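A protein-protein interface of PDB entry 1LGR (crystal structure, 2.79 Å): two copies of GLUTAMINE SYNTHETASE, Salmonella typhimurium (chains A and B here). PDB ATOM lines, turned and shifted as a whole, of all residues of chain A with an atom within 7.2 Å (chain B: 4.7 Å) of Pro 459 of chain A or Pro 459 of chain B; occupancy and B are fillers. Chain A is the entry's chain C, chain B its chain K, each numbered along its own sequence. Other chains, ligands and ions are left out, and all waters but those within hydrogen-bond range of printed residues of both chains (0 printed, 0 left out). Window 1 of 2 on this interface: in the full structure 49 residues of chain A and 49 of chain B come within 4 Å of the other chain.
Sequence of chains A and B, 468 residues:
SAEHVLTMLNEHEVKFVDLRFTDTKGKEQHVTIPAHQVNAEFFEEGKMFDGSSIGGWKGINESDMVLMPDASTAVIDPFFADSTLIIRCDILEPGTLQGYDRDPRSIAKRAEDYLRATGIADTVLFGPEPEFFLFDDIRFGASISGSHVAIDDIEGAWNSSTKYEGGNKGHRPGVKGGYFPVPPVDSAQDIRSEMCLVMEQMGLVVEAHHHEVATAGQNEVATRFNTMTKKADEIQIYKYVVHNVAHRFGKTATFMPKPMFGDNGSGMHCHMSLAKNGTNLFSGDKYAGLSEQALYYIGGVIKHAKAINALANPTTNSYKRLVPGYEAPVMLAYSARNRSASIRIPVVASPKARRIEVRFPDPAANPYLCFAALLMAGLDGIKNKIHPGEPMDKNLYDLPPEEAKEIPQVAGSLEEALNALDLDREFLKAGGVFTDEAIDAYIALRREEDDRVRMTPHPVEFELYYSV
Of chain B, only Ser 147 (3.5 Å), His 148 (3.6 Å) and Pro 459 (3.7 Å) come within 4 Å of Pro 459 of chain A. Printed residues of chain B within 4 Å of His 458 of chain A: Pro 457 (3.5 Å) and His 458 (3.6 Å). Printed residues of chain B within 4 Å of Gly 146 of chain A: Val 149 (3.2 Å). Gly 141 of chain A touches none of the printed residues of chain B. Gly 141 of chain B touches none of the printed residues of chain A. The nearest printed residue of chain B that does not touch Met 256 of chain A is Glu 461 of chain B (4.2 Å).
Hydrophobic or aromatic side chains of chain B that line the printed part of chain A: His 148, Val 149, His 458, Pro 459, Val 460 and Phe 462. Along chain B the printed residues that touch a printed residue of chain A span positions 147 to 463. Among the printed residues, Asp or Glu carboxylates within 4 Å of a Lys or Arg side-chain nitrogen of the other chain: Arg 452 of chain A with Glu 463 of chain B (2.9 Å).
O of Ser 147 of chain A sits at hydrogen-bond distance from N of Val 149 of chain B. O of Ser 147 of chain B is in hydrogen-bond range of N of Val 149 of chain A (2.9 Å). NH2 of Arg 452 of chain A lies within salt-bridge range of OE2 of Glu 463 of chain B (2.9 Å).
His 148 of chain B touches its own counterpart, His 148 of chain A. His 148 of chain A touches Pro 459 of chain B, and with the chains exchanged Pro 459 of chain A touches His 148 of chain B. Pro 457 of chain A touches His 458 of chain B, and with the chains exchanged His 458 of chain A touches Pro 457 of chain B. Pro 459 of chain B touches its own counterpart, Pro 459 of chain A. Of the 25 pairs that touch across the chains among the printed residues, 15 have their exchanged pair printed and touching as well.
Val 460 of chain B touches Ala 142 of chain A. O of His 148 of chain A touches CB of Pro 459 of chain B, at 3.6 Å. Val 149 of chain A touches Phe 462 of chain B (CG2 to CD1, 3.4 Å). Phe 462 of chain B touches Met 256 of chain A. O of Thr 456 of chain A touches CE1 of His 458 of chain B, at 2.9 Å. Thr 456 of chain A touches Val 460 of chain B. CE1 of His 458 of chain B touches O of Pro 457 of chain A (3.5 Å). ND1 of His 458 of chain A touches ND1 of His 458 of chain B, at 3.6 Å. OG of Ser 147 of chain B touches CG of Pro 459 of chain A, 3.5 Å away. His 148 of chain B touches Pro 459 of chain A.
The backbone carbonyl oxygen (O) of Gly 141 of chain A lies within hydrogen-bond range of the backbone NH (N) of His 148 of chain A (2.7 Å). OG1 of Thr 456 of chain A lies within hydrogen-bond range of O of Arg 452 of chain A. The side-chain carboxylate (OE1) of Glu 461 of chain A is in hydrogen-bond range of the backbone NH (N) of His 458 of chain A (3.1 Å). The backbone NH (N) of His 148 of chain B is in hydrogen-bond range of the backbone carbonyl oxygen (O) of Gly 141 of chain B. N of His 458 of chain B sits at hydrogen-bond distance from OE1 of Glu 461 of chain B, 3.1 Å away.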
ATOM      1  N   PHE A 140      -0.591  19.715  15.962  1.00  0.00           N
ATOM      2  CA  PHE A 140       0.625  19.591  15.189  1.00  0.00           C
ATOM      3  C   PHE A 140       0.323  19.151  13.766  1.00  0.00           C
ATOM      4  O   PHE A 140      -0.778  18.706  13.442  1.00  0.00           O
ATOM      5  CB  PHE A 140       1.589  18.581  15.804  1.00  0.00           C
ATOM      6  CG  PHE A 140       0.977  17.223  16.088  1.00  0.00           C
ATOM      7  CD1 PHE A 140       0.842  16.280  15.060  1.00  0.00           C
ATOM      8  CD2 PHE A 140       0.537  16.930  17.384  1.00  0.00           C
ATOM      9  CE1 PHE A 140       0.255  15.055  15.327  1.00  0.00           C
ATOM     10  CE2 PHE A 140      -0.037  15.684  17.650  1.00  0.00           C
ATOM     11  CZ  PHE A 140      -0.179  14.757  16.617  1.00  0.00           C
ATOM     12  N   GLY A 141       1.289  19.323  12.883  1.00  0.00           N
ATOM     13  CA  GLY A 141       1.102  18.929  11.501  1.00  0.00           C
ATOM     14  C   GLY A 141       2.351  19.195  10.688  1.00  0.00           C
ATOM     15  O   GLY A 141       3.164  20.064  11.009  1.00  0.00           O
ATOM     16  N   ALA A 142       2.498  18.436   9.626  1.00  0.00           N
ATOM     17  CA  ALA A 142       3.582  18.581   8.671  1.00  0.00           C
ATOM     18  C   ALA A 142       2.935  18.408   7.270  1.00  0.00           C
ATOM     19  O   ALA A 142       2.010  17.604   7.053  1.00  0.00           O
ATOM     20  CB  ALA A 142       4.612  17.496   8.895  1.00  0.00           C
ATOM     21  N   GLY A 146       5.181  23.423   5.070  1.00  0.00           N
ATOM     22  CA  GLY A 146       5.562  23.701   6.456  1.00  0.00           C
ATOM     23  C   GLY A 146       5.237  22.606   7.506  1.00  0.00           C
ATOM     24  O   GLY A 146       4.724  21.499   7.238  1.00  0.00           O
ATOM     25  N   SER A 147       5.530  22.944   8.755  1.00  0.00           N
ATOM     26  CA  SER A 147       5.236  22.027   9.831  1.00  0.00           C
ATOM     27  C   SER A 147       5.150  22.750  11.160  1.00  0.00           C
ATOM     28  O   SER A 147       5.686  23.854  11.320  1.00  0.00           O
ATOM     29  CB  SER A 147       6.286  20.923   9.982  1.00  0.00           C
ATOM     30  OG  SER A 147       7.611  21.340  10.235  1.00  0.00           O
ATOM     31  N   HIS A 148       4.459  22.170  12.143  1.00  0.00           N
ATOM     32  CA  HIS A 148       4.266  22.802  13.437  1.00  0.00           C
ATOM     33  C   HIS A 148       3.816  21.864  14.527  1.00  0.00           C
ATOM     34  O   HIS A 148       3.183  20.852  14.266  1.00  0.00           O
ATOM     35  CB  HIS A 148       3.207  23.897  13.392  1.00  0.00           C
ATOM     36  CG  HIS A 148       1.768  23.422  13.242  1.00  0.00           C
ATOM     37  ND1 HIS A 148       1.192  22.805  12.221  1.00  0.00           N
ATOM     38  CD2 HIS A 148       0.814  23.561  14.232  1.00  0.00           C
ATOM     39  CE1 HIS A 148      -0.058  22.572  12.539  1.00  0.00           C
ATOM     40  NE2 HIS A 148      -0.274  23.032  13.746  1.00  0.00           N
ATOM     41  N   VAL A 149       4.058  22.292  15.746  1.00  0.00           N
ATOM     42  CA  VAL A 149       3.462  21.682  16.927  1.00  0.00           C
ATOM     43  C   VAL A 149       3.205  22.826  17.918  1.00  0.00           C
ATOM     44  O   VAL A 149       3.980  23.781  18.052  1.00  0.00           O
ATOM     45  CB  VAL A 149       4.391  20.609  17.545  1.00  0.00           C
ATOM     46  CG1 VAL A 149       5.748  21.178  17.890  1.00  0.00           C
ATOM     47  CG2 VAL A 149       3.689  20.030  18.767  1.00  0.00           C
ATOM     48  N   MET A 256       5.118  10.681  25.547  1.00  0.00           N
ATOM     49  CA  MET A 256       6.333  10.863  24.771  1.00  0.00           C
ATOM     50  C   MET A 256       7.433  11.517  25.613  1.00  0.00           C
ATOM     51  O   MET A 256       7.178  12.303  26.534  1.00  0.00           O
ATOM     52  CB  MET A 256       6.031  11.676  23.497  1.00  0.00           C
ATOM     53  CG  MET A 256       5.904  13.178  23.513  1.00  0.00           C
ATOM     54  SD  MET A 256       5.465  13.792  21.878  1.00  0.00           S
ATOM     55  CE  MET A 256       7.053  14.149  21.223  1.00  0.00           C
ATOM     56  N   ARG A 452      11.723   9.555   8.412  1.00  0.00           N
ATOM     57  CA  ARG A 452      10.751  10.640   8.304  1.00  0.00           C
ATOM     58  C   ARG A 452      11.211  11.859   9.112  1.00  0.00           C
ATOM     59  O   ARG A 452      11.266  12.994   8.633  1.00  0.00           O
ATOM     60  CB  ARG A 452       9.405  10.093   8.780  1.00  0.00           C
ATOM     61  CG  ARG A 452       8.343  11.154   8.701  1.00  0.00           C
ATOM     62  CD  ARG A 452       6.936  10.688   8.356  1.00  0.00           C
ATOM     63  NE  ARG A 452       5.995  11.750   8.674  1.00  0.00           N
ATOM     64  CZ  ARG A 452       6.003  12.979   8.118  1.00  0.00           C
ATOM     65  NH1 ARG A 452       6.834  13.378   7.139  1.00  0.00           N
ATOM     66  NH2 ARG A 452       5.109  13.857   8.559  1.00  0.00           N
ATOM     67  N   THR A 456      12.610  15.422   6.985  1.00  0.00           N
ATOM     68  CA  THR A 456      11.699  16.557   7.088  1.00  0.00           C
ATOM     69  C   THR A 456      12.399  17.767   7.683  1.00  0.00           C
ATOM     70  O   THR A 456      12.828  17.714   8.841  1.00  0.00           O
ATOM     71  CB  THR A 456      10.469  16.194   7.957  1.00  0.00           C
ATOM     72  OG1 THR A 456       9.691  15.236   7.242  1.00  0.00           O
ATOM     73  CG2 THR A 456       9.585  17.393   8.225  1.00  0.00           C
ATOM     74  N   PRO A 457      12.543  18.916   7.010  1.00  0.00           N
ATOM     75  CA  PRO A 457      13.141  20.111   7.603  1.00  0.00           C
ATOM     76  C   PRO A 457      12.474  20.581   8.878  1.00  0.00           C
ATOM     77  O   PRO A 457      11.278  20.523   9.133  1.00  0.00           O
ATOM     78  CB  PRO A 457      13.134  21.129   6.469  1.00  0.00           C
ATOM     79  CG  PRO A 457      12.148  20.604   5.466  1.00  0.00           C
ATOM     80  CD  PRO A 457      12.293  19.105   5.579  1.00  0.00           C
ATOM     81  N   HIS A 458      13.363  20.860   9.811  1.00  0.00           N
ATOM     82  CA  HIS A 458      12.990  21.257  11.166  1.00  0.00           C
ATOM     83  C   HIS A 458      12.756  22.762  11.229  1.00  0.00           C
ATOM     84  O   HIS A 458      13.616  23.501  10.746  1.00  0.00           O
ATOM     85  CB  HIS A 458      14.121  20.893  12.146  1.00  0.00           C
ATOM     86  CG  HIS A 458      13.800  21.006  13.630  1.00  0.00           C
ATOM     87  ND1 HIS A 458      13.859  20.040  14.539  1.00  0.00           N
ATOM     88  CD2 HIS A 458      13.372  22.127  14.287  1.00  0.00           C
ATOM     89  CE1 HIS A 458      13.471  20.530  15.696  1.00  0.00           C
ATOM     90  NE2 HIS A 458      13.184  21.793  15.529  1.00  0.00           N
ATOM     91  N   PRO A 459      11.732  23.273  11.924  1.00  0.00           N
ATOM     92  CA  PRO A 459      11.608  24.696  12.194  1.00  0.00           C
ATOM     93  C   PRO A 459      12.863  25.420  12.689  1.00  0.00           C
ATOM     94  O   PRO A 459      13.227  26.376  12.006  1.00  0.00           O
ATOM     95  CB  PRO A 459      10.451  24.797  13.158  1.00  0.00           C
ATOM     96  CG  PRO A 459       9.940  23.408  13.359  1.00  0.00           C
ATOM     97  CD  PRO A 459      10.457  22.621  12.164  1.00  0.00           C
ATOM     98  N   VAL A 460      13.652  25.063  13.730  1.00  0.00           N
ATOM     99  CA  VAL A 460      14.844  25.879  14.027  1.00  0.00           C
ATOM    100  C   VAL A 460      15.889  25.931  12.890  1.00  0.00           C
ATOM    101  O   VAL A 460      16.727  26.831  12.855  1.00  0.00           O
ATOM    102  CB  VAL A 460      15.578  25.434  15.344  1.00  0.00           C
ATOM    103  CG1 VAL A 460      14.520  25.207  16.403  1.00  0.00           C
ATOM    104  CG2 VAL A 460      16.416  24.210  15.179  1.00  0.00           C
ATOM    105  N   GLU A 461      15.832  25.051  11.874  1.00  0.00           N
ATOM    106  CA  GLU A 461      16.722  25.180  10.718  1.00  0.00           C
ATOM    107  C   GLU A 461      16.356  26.466   9.965  1.00  0.00           C
ATOM    108  O   GLU A 461      17.260  27.172   9.526  1.00  0.00           O
ATOM    109  CB  GLU A 461      16.595  24.008   9.747  1.00  0.00           C
ATOM    110  CG  GLU A 461      17.038  22.725  10.408  1.00  0.00           C
ATOM    111  CD  GLU A 461      17.051  21.475   9.533  1.00  0.00           C
ATOM    112  OE1 GLU A 461      16.220  21.330   8.635  1.00  0.00           O
ATOM    113  OE2 GLU A 461      17.906  20.625   9.765  1.00  0.00           O
ATOM    114  N   PHE A 462      15.084  26.875   9.854  1.00  0.00           N
ATOM    115  CA  PHE A 462      14.777  28.157   9.232  1.00  0.00           C
ATOM    116  C   PHE A 462      15.323  29.308  10.064  1.00  0.00           C
ATOM    117  O   PHE A 462      15.897  30.268   9.548  1.00  0.00           O
ATOM    118  CB  PHE A 462      13.297  28.315   9.076  1.00  0.00           C
ATOM    119  CG  PHE A 462      12.865  27.443   7.926  1.00  0.00           C
ATOM    120  CD1 PHE A 462      12.618  26.092   8.135  1.00  0.00           C
ATOM    121  CD2 PHE A 462      12.768  27.990   6.646  1.00  0.00           C
ATOM    122  CE1 PHE A 462      12.277  25.275   7.075  1.00  0.00           C
ATOM    123  CE2 PHE A 462      12.427  27.165   5.574  1.00  0.00           C
ATOM    124  CZ  PHE A 462      12.183  25.808   5.800  1.00  0.00           C
ATOM    125  N   GLU A 463      15.278  29.138  11.387  1.00  0.00           N
ATOM    126  CA  GLU A 463      15.843  30.122  12.311  1.00  0.00           C
ATOM    127  C   GLU A 463      17.354  30.319  12.133  1.00  0.00           C
ATOM    128  O   GLU A 463      17.896  31.422  12.114  1.00  0.00           O
ATOM    129  CB  GLU A 463      15.549  29.650  13.694  1.00  0.00           C
ATOM    130  CG  GLU A 463      15.513  30.787  14.646  1.00  0.00           C
ATOM    131  CD  GLU A 463      15.275  30.251  16.053  1.00  0.00           C
ATOM    132  OE1 GLU A 463      14.107  30.040  16.417  1.00  0.00           O
ATOM    133  OE2 GLU A 463      16.270  30.030  16.757  1.00  0.00           O
ATOM    134  N   LEU A 464      18.006  29.186  11.929  1.00  0.00           N
ATOM    135  CA  LEU A 464      19.444  29.077  11.744  1.00  0.00           C
ATOM    136  C   LEU A 464      19.998  29.409  10.364  1.00  0.00           C
ATOM    137  O   LEU A 464      21.002  30.088  10.165  1.00  0.00           O
ATOM    138  CB  LEU A 464      19.828  27.652  12.118  1.00  0.00           C
ATOM    139  CG  LEU A 464      20.539  27.343  13.429  1.00  0.00           C
ATOM    140  CD1 LEU A 464      20.135  28.288  14.531  1.00  0.00           C
ATOM    141  CD2 LEU A 464      20.207  25.922  13.802  1.00  0.00           C
ATOM    142  N   TYR A 465      19.291  28.919   9.360  1.00  0.00           N
ATOM    143  CA  TYR A 465      19.777  28.949   7.989  1.00  0.00           C
ATOM    144  C   TYR A 465      18.951  29.672   6.936  1.00  0.00           C
ATOM    145  O   TYR A 465      19.367  29.679   5.781  1.00  0.00           O
ATOM    146  CB  TYR A 465      19.988  27.514   7.510  1.00  0.00           C
ATOM    147  CG  TYR A 465      20.805  26.676   8.460  1.00  0.00           C
ATOM    148  CD1 TYR A 465      22.067  27.091   8.855  1.00  0.00           C
ATOM    149  CD2 TYR A 465      20.278  25.486   8.926  1.00  0.00           C
ATOM    150  CE1 TYR A 465      22.815  26.305   9.717  1.00  0.00           C
ATOM    151  CE2 TYR A 465      21.018  24.696   9.787  1.00  0.00           C
ATOM    152  CZ  TYR A 465      22.291  25.100  10.173  1.00  0.00           C
ATOM    153  OH  TYR A 465      23.066  24.243  10.933  1.00  0.00           O
ATOM    154  N   GLY B 141       9.197  29.915  13.874  1.00  0.00           N
ATOM    155  CA  GLY B 141       9.486  30.237  15.256  1.00  0.00           C
ATOM    156  C   GLY B 141       9.558  28.982  16.100  1.00  0.00           C
ATOM    157  O   GLY B 141       8.960  27.951  15.788  1.00  0.00           O
ATOM    158  N   SER B 147       6.796  24.928  18.057  1.00  0.00           N
ATOM    159  CA  SER B 147       7.621  25.441  16.990  1.00  0.00           C
ATOM    160  C   SER B 147       6.937  25.291  15.645  1.00  0.00           C
ATOM    161  O   SER B 147       6.030  24.466  15.483  1.00  0.00           O
ATOM    162  CB  SER B 147       8.979  24.738  16.890  1.00  0.00           C
ATOM    163  OG  SER B 147       8.953  23.345  16.668  1.00  0.00           O
ATOM    164  N   HIS B 148       7.325  26.095  14.654  1.00  0.00           N
ATOM    165  CA  HIS B 148       6.700  26.074  13.344  1.00  0.00           C
ATOM    166  C   HIS B 148       7.502  26.742  12.259  1.00  0.00           C
ATOM    167  O   HIS B 148       8.291  27.638  12.519  1.00  0.00           O
ATOM    168  CB  HIS B 148       5.352  26.785  13.339  1.00  0.00           C
ATOM    169  CG  HIS B 148       5.404  28.303  13.455  1.00  0.00           C
ATOM    170  ND1 HIS B 148       5.810  29.052  14.470  1.00  0.00           N
ATOM    171  CD2 HIS B 148       5.029  29.157  12.434  1.00  0.00           C
ATOM    172  CE1 HIS B 148       5.693  30.309  14.119  1.00  0.00           C
ATOM    173  NE2 HIS B 148       5.221  30.361  12.898  1.00  0.00           N
ATOM    174  N   VAL B 149       7.191  26.362  11.039  1.00  0.00           N
ATOM    175  CA  VAL B 149       7.638  27.078   9.853  1.00  0.00           C
ATOM    176  C   VAL B 149       6.495  26.982   8.834  1.00  0.00           C
ATOM    177  O   VAL B 149       5.797  25.968   8.706  1.00  0.00           O
ATOM    178  CB  VAL B 149       8.945  26.470   9.281  1.00  0.00           C
ATOM    179  CG1 VAL B 149       8.784  25.001   8.966  1.00  0.00           C
ATOM    180  CG2 VAL B 149       9.335  27.278   8.050  1.00  0.00           C
ATOM    181  N   PRO B 457      12.572  19.360  20.080  1.00  0.00           N
ATOM    182  CA  PRO B 457      11.607  18.439  19.482  1.00  0.00           C
ATOM    183  C   PRO B 457      11.002  18.918  18.180  1.00  0.00           C
ATOM    184  O   PRO B 457      10.730  20.076  17.891  1.00  0.00           O
ATOM    185  CB  PRO B 457      10.599  18.187  20.597  1.00  0.00           C
ATOM    186  CG  PRO B 457      10.802  19.304  21.580  1.00  0.00           C
ATOM    187  CD  PRO B 457      12.285  19.581  21.498  1.00  0.00           C
ATOM    188  N   HIS B 458      11.006  17.966  17.268  1.00  0.00           N
ATOM    189  CA  HIS B 458      10.555  18.181  15.896  1.00  0.00           C
ATOM    190  C   HIS B 458       9.047  17.984  15.799  1.00  0.00           C
ATOM    191  O   HIS B 458       8.566  16.964  16.294  1.00  0.00           O
ATOM    192  CB  HIS B 458      11.245  17.176  14.957  1.00  0.00           C
ATOM    193  CG  HIS B 458      11.085  17.417  13.462  1.00  0.00           C
ATOM    194  ND1 HIS B 458      12.051  17.609  12.573  1.00  0.00           N
ATOM    195  CD2 HIS B 458       9.906  17.499  12.773  1.00  0.00           C
ATOM    196  CE1 HIS B 458      11.503  17.819  11.397  1.00  0.00           C
ATOM    197  NE2 HIS B 458      10.206  17.744  11.532  1.00  0.00           N
ATOM    198  N   PRO B 459       8.288  18.809  15.065  1.00  0.00           N
ATOM    199  CA  PRO B 459       6.894  18.525  14.767  1.00  0.00           C
ATOM    200  C   PRO B 459       6.561  17.108  14.295  1.00  0.00           C
ATOM    201  O   PRO B 459       5.728  16.506  14.972  1.00  0.00           O
ATOM    202  CB  PRO B 459       6.500  19.584  13.768  1.00  0.00           C
ATOM    203  CG  PRO B 459       7.696  20.459  13.577  1.00  0.00           C
ATOM    204  CD  PRO B 459       8.565  20.210  14.800  1.00  0.00           C
ATOM    205  N   VAL B 460       7.151  16.425  13.285  1.00  0.00           N
ATOM    206  CA  VAL B 460       6.707  15.046  13.008  1.00  0.00           C
ATOM    207  C   VAL B 460       6.918  14.054  14.174  1.00  0.00           C
ATOM    208  O   VAL B 460       6.288  12.999  14.217  1.00  0.00           O
ATOM    209  CB  VAL B 460       7.372  14.434  11.721  1.00  0.00           C
ATOM    210  CG1 VAL B 460       7.323  15.489  10.636  1.00  0.00           C
ATOM    211  CG2 VAL B 460       8.777  13.976  11.933  1.00  0.00           C
ATOM    212  N   GLU B 461       7.723  14.378  15.203  1.00  0.00           N
ATOM    213  CA  GLU B 461       7.817  13.514  16.382  1.00  0.00           C
ATOM    214  C   GLU B 461       6.461  13.523  17.100  1.00  0.00           C
ATOM    215  O   GLU B 461       6.023  12.469  17.554  1.00  0.00           O
ATOM    216  CB  GLU B 461       8.882  13.986  17.369  1.00  0.00           C
ATOM    217  CG  GLU B 461      10.254  13.904  16.746  1.00  0.00           C
ATOM    218  CD  GLU B 461      11.435  14.260  17.643  1.00  0.00           C
ATOM    219  OE1 GLU B 461      11.321  15.119  18.518  1.00  0.00           O
ATOM    220  OE2 GLU B 461      12.495  13.671  17.451  1.00  0.00           O
ATOM    221  N   PHE B 462       5.711  14.633  17.168  1.00  0.00           N
ATOM    222  CA  PHE B 462       4.379  14.584  17.758  1.00  0.00           C
ATOM    223  C   PHE B 462       3.448  13.720  16.921  1.00  0.00           C
ATOM    224  O   PHE B 462       2.673  12.913  17.435  1.00  0.00           O
ATOM    225  CB  PHE B 462       3.811  15.965  17.867  1.00  0.00           C
ATOM    226  CG  PHE B 462       4.499  16.649  19.019  1.00  0.00           C
ATOM    227  CD1 PHE B 462       5.732  17.258  18.827  1.00  0.00           C
ATOM    228  CD2 PHE B 462       3.912  16.620  20.285  1.00  0.00           C
ATOM    229  CE1 PHE B 462       6.394  17.839  19.890  1.00  0.00           C
ATOM    230  CE2 PHE B 462       4.584  17.201  21.361  1.00  0.00           C
ATOM    231  CZ  PHE B 462       5.824  17.810  21.153  1.00  0.00           C
ATOM    232  N   GLU B 463       3.632  13.780  15.600  1.00  0.00           N
ATOM    233  CA  GLU B 463       2.868  12.942  14.675  1.00  0.00           C
ATOM    234  C   GLU B 463       3.095  11.441  14.894  1.00  0.00           C
ATOM    235  O   GLU B 463       2.187  10.612  14.909  1.00  0.00           O
ATOM    236  CB  GLU B 463       3.275  13.325  13.293  1.00  0.00           C
ATOM    237  CG  GLU B 463       2.197  13.019  12.320  1.00  0.00           C
ATOM    238  CD  GLU B 463       2.682  13.365  10.917  1.00  0.00           C
ATOM    239  OE1 GLU B 463       2.569  14.536  10.522  1.00  0.00           O
ATOM    240  OE2 GLU B 463       3.188  12.455  10.246  1.00  0.00           O
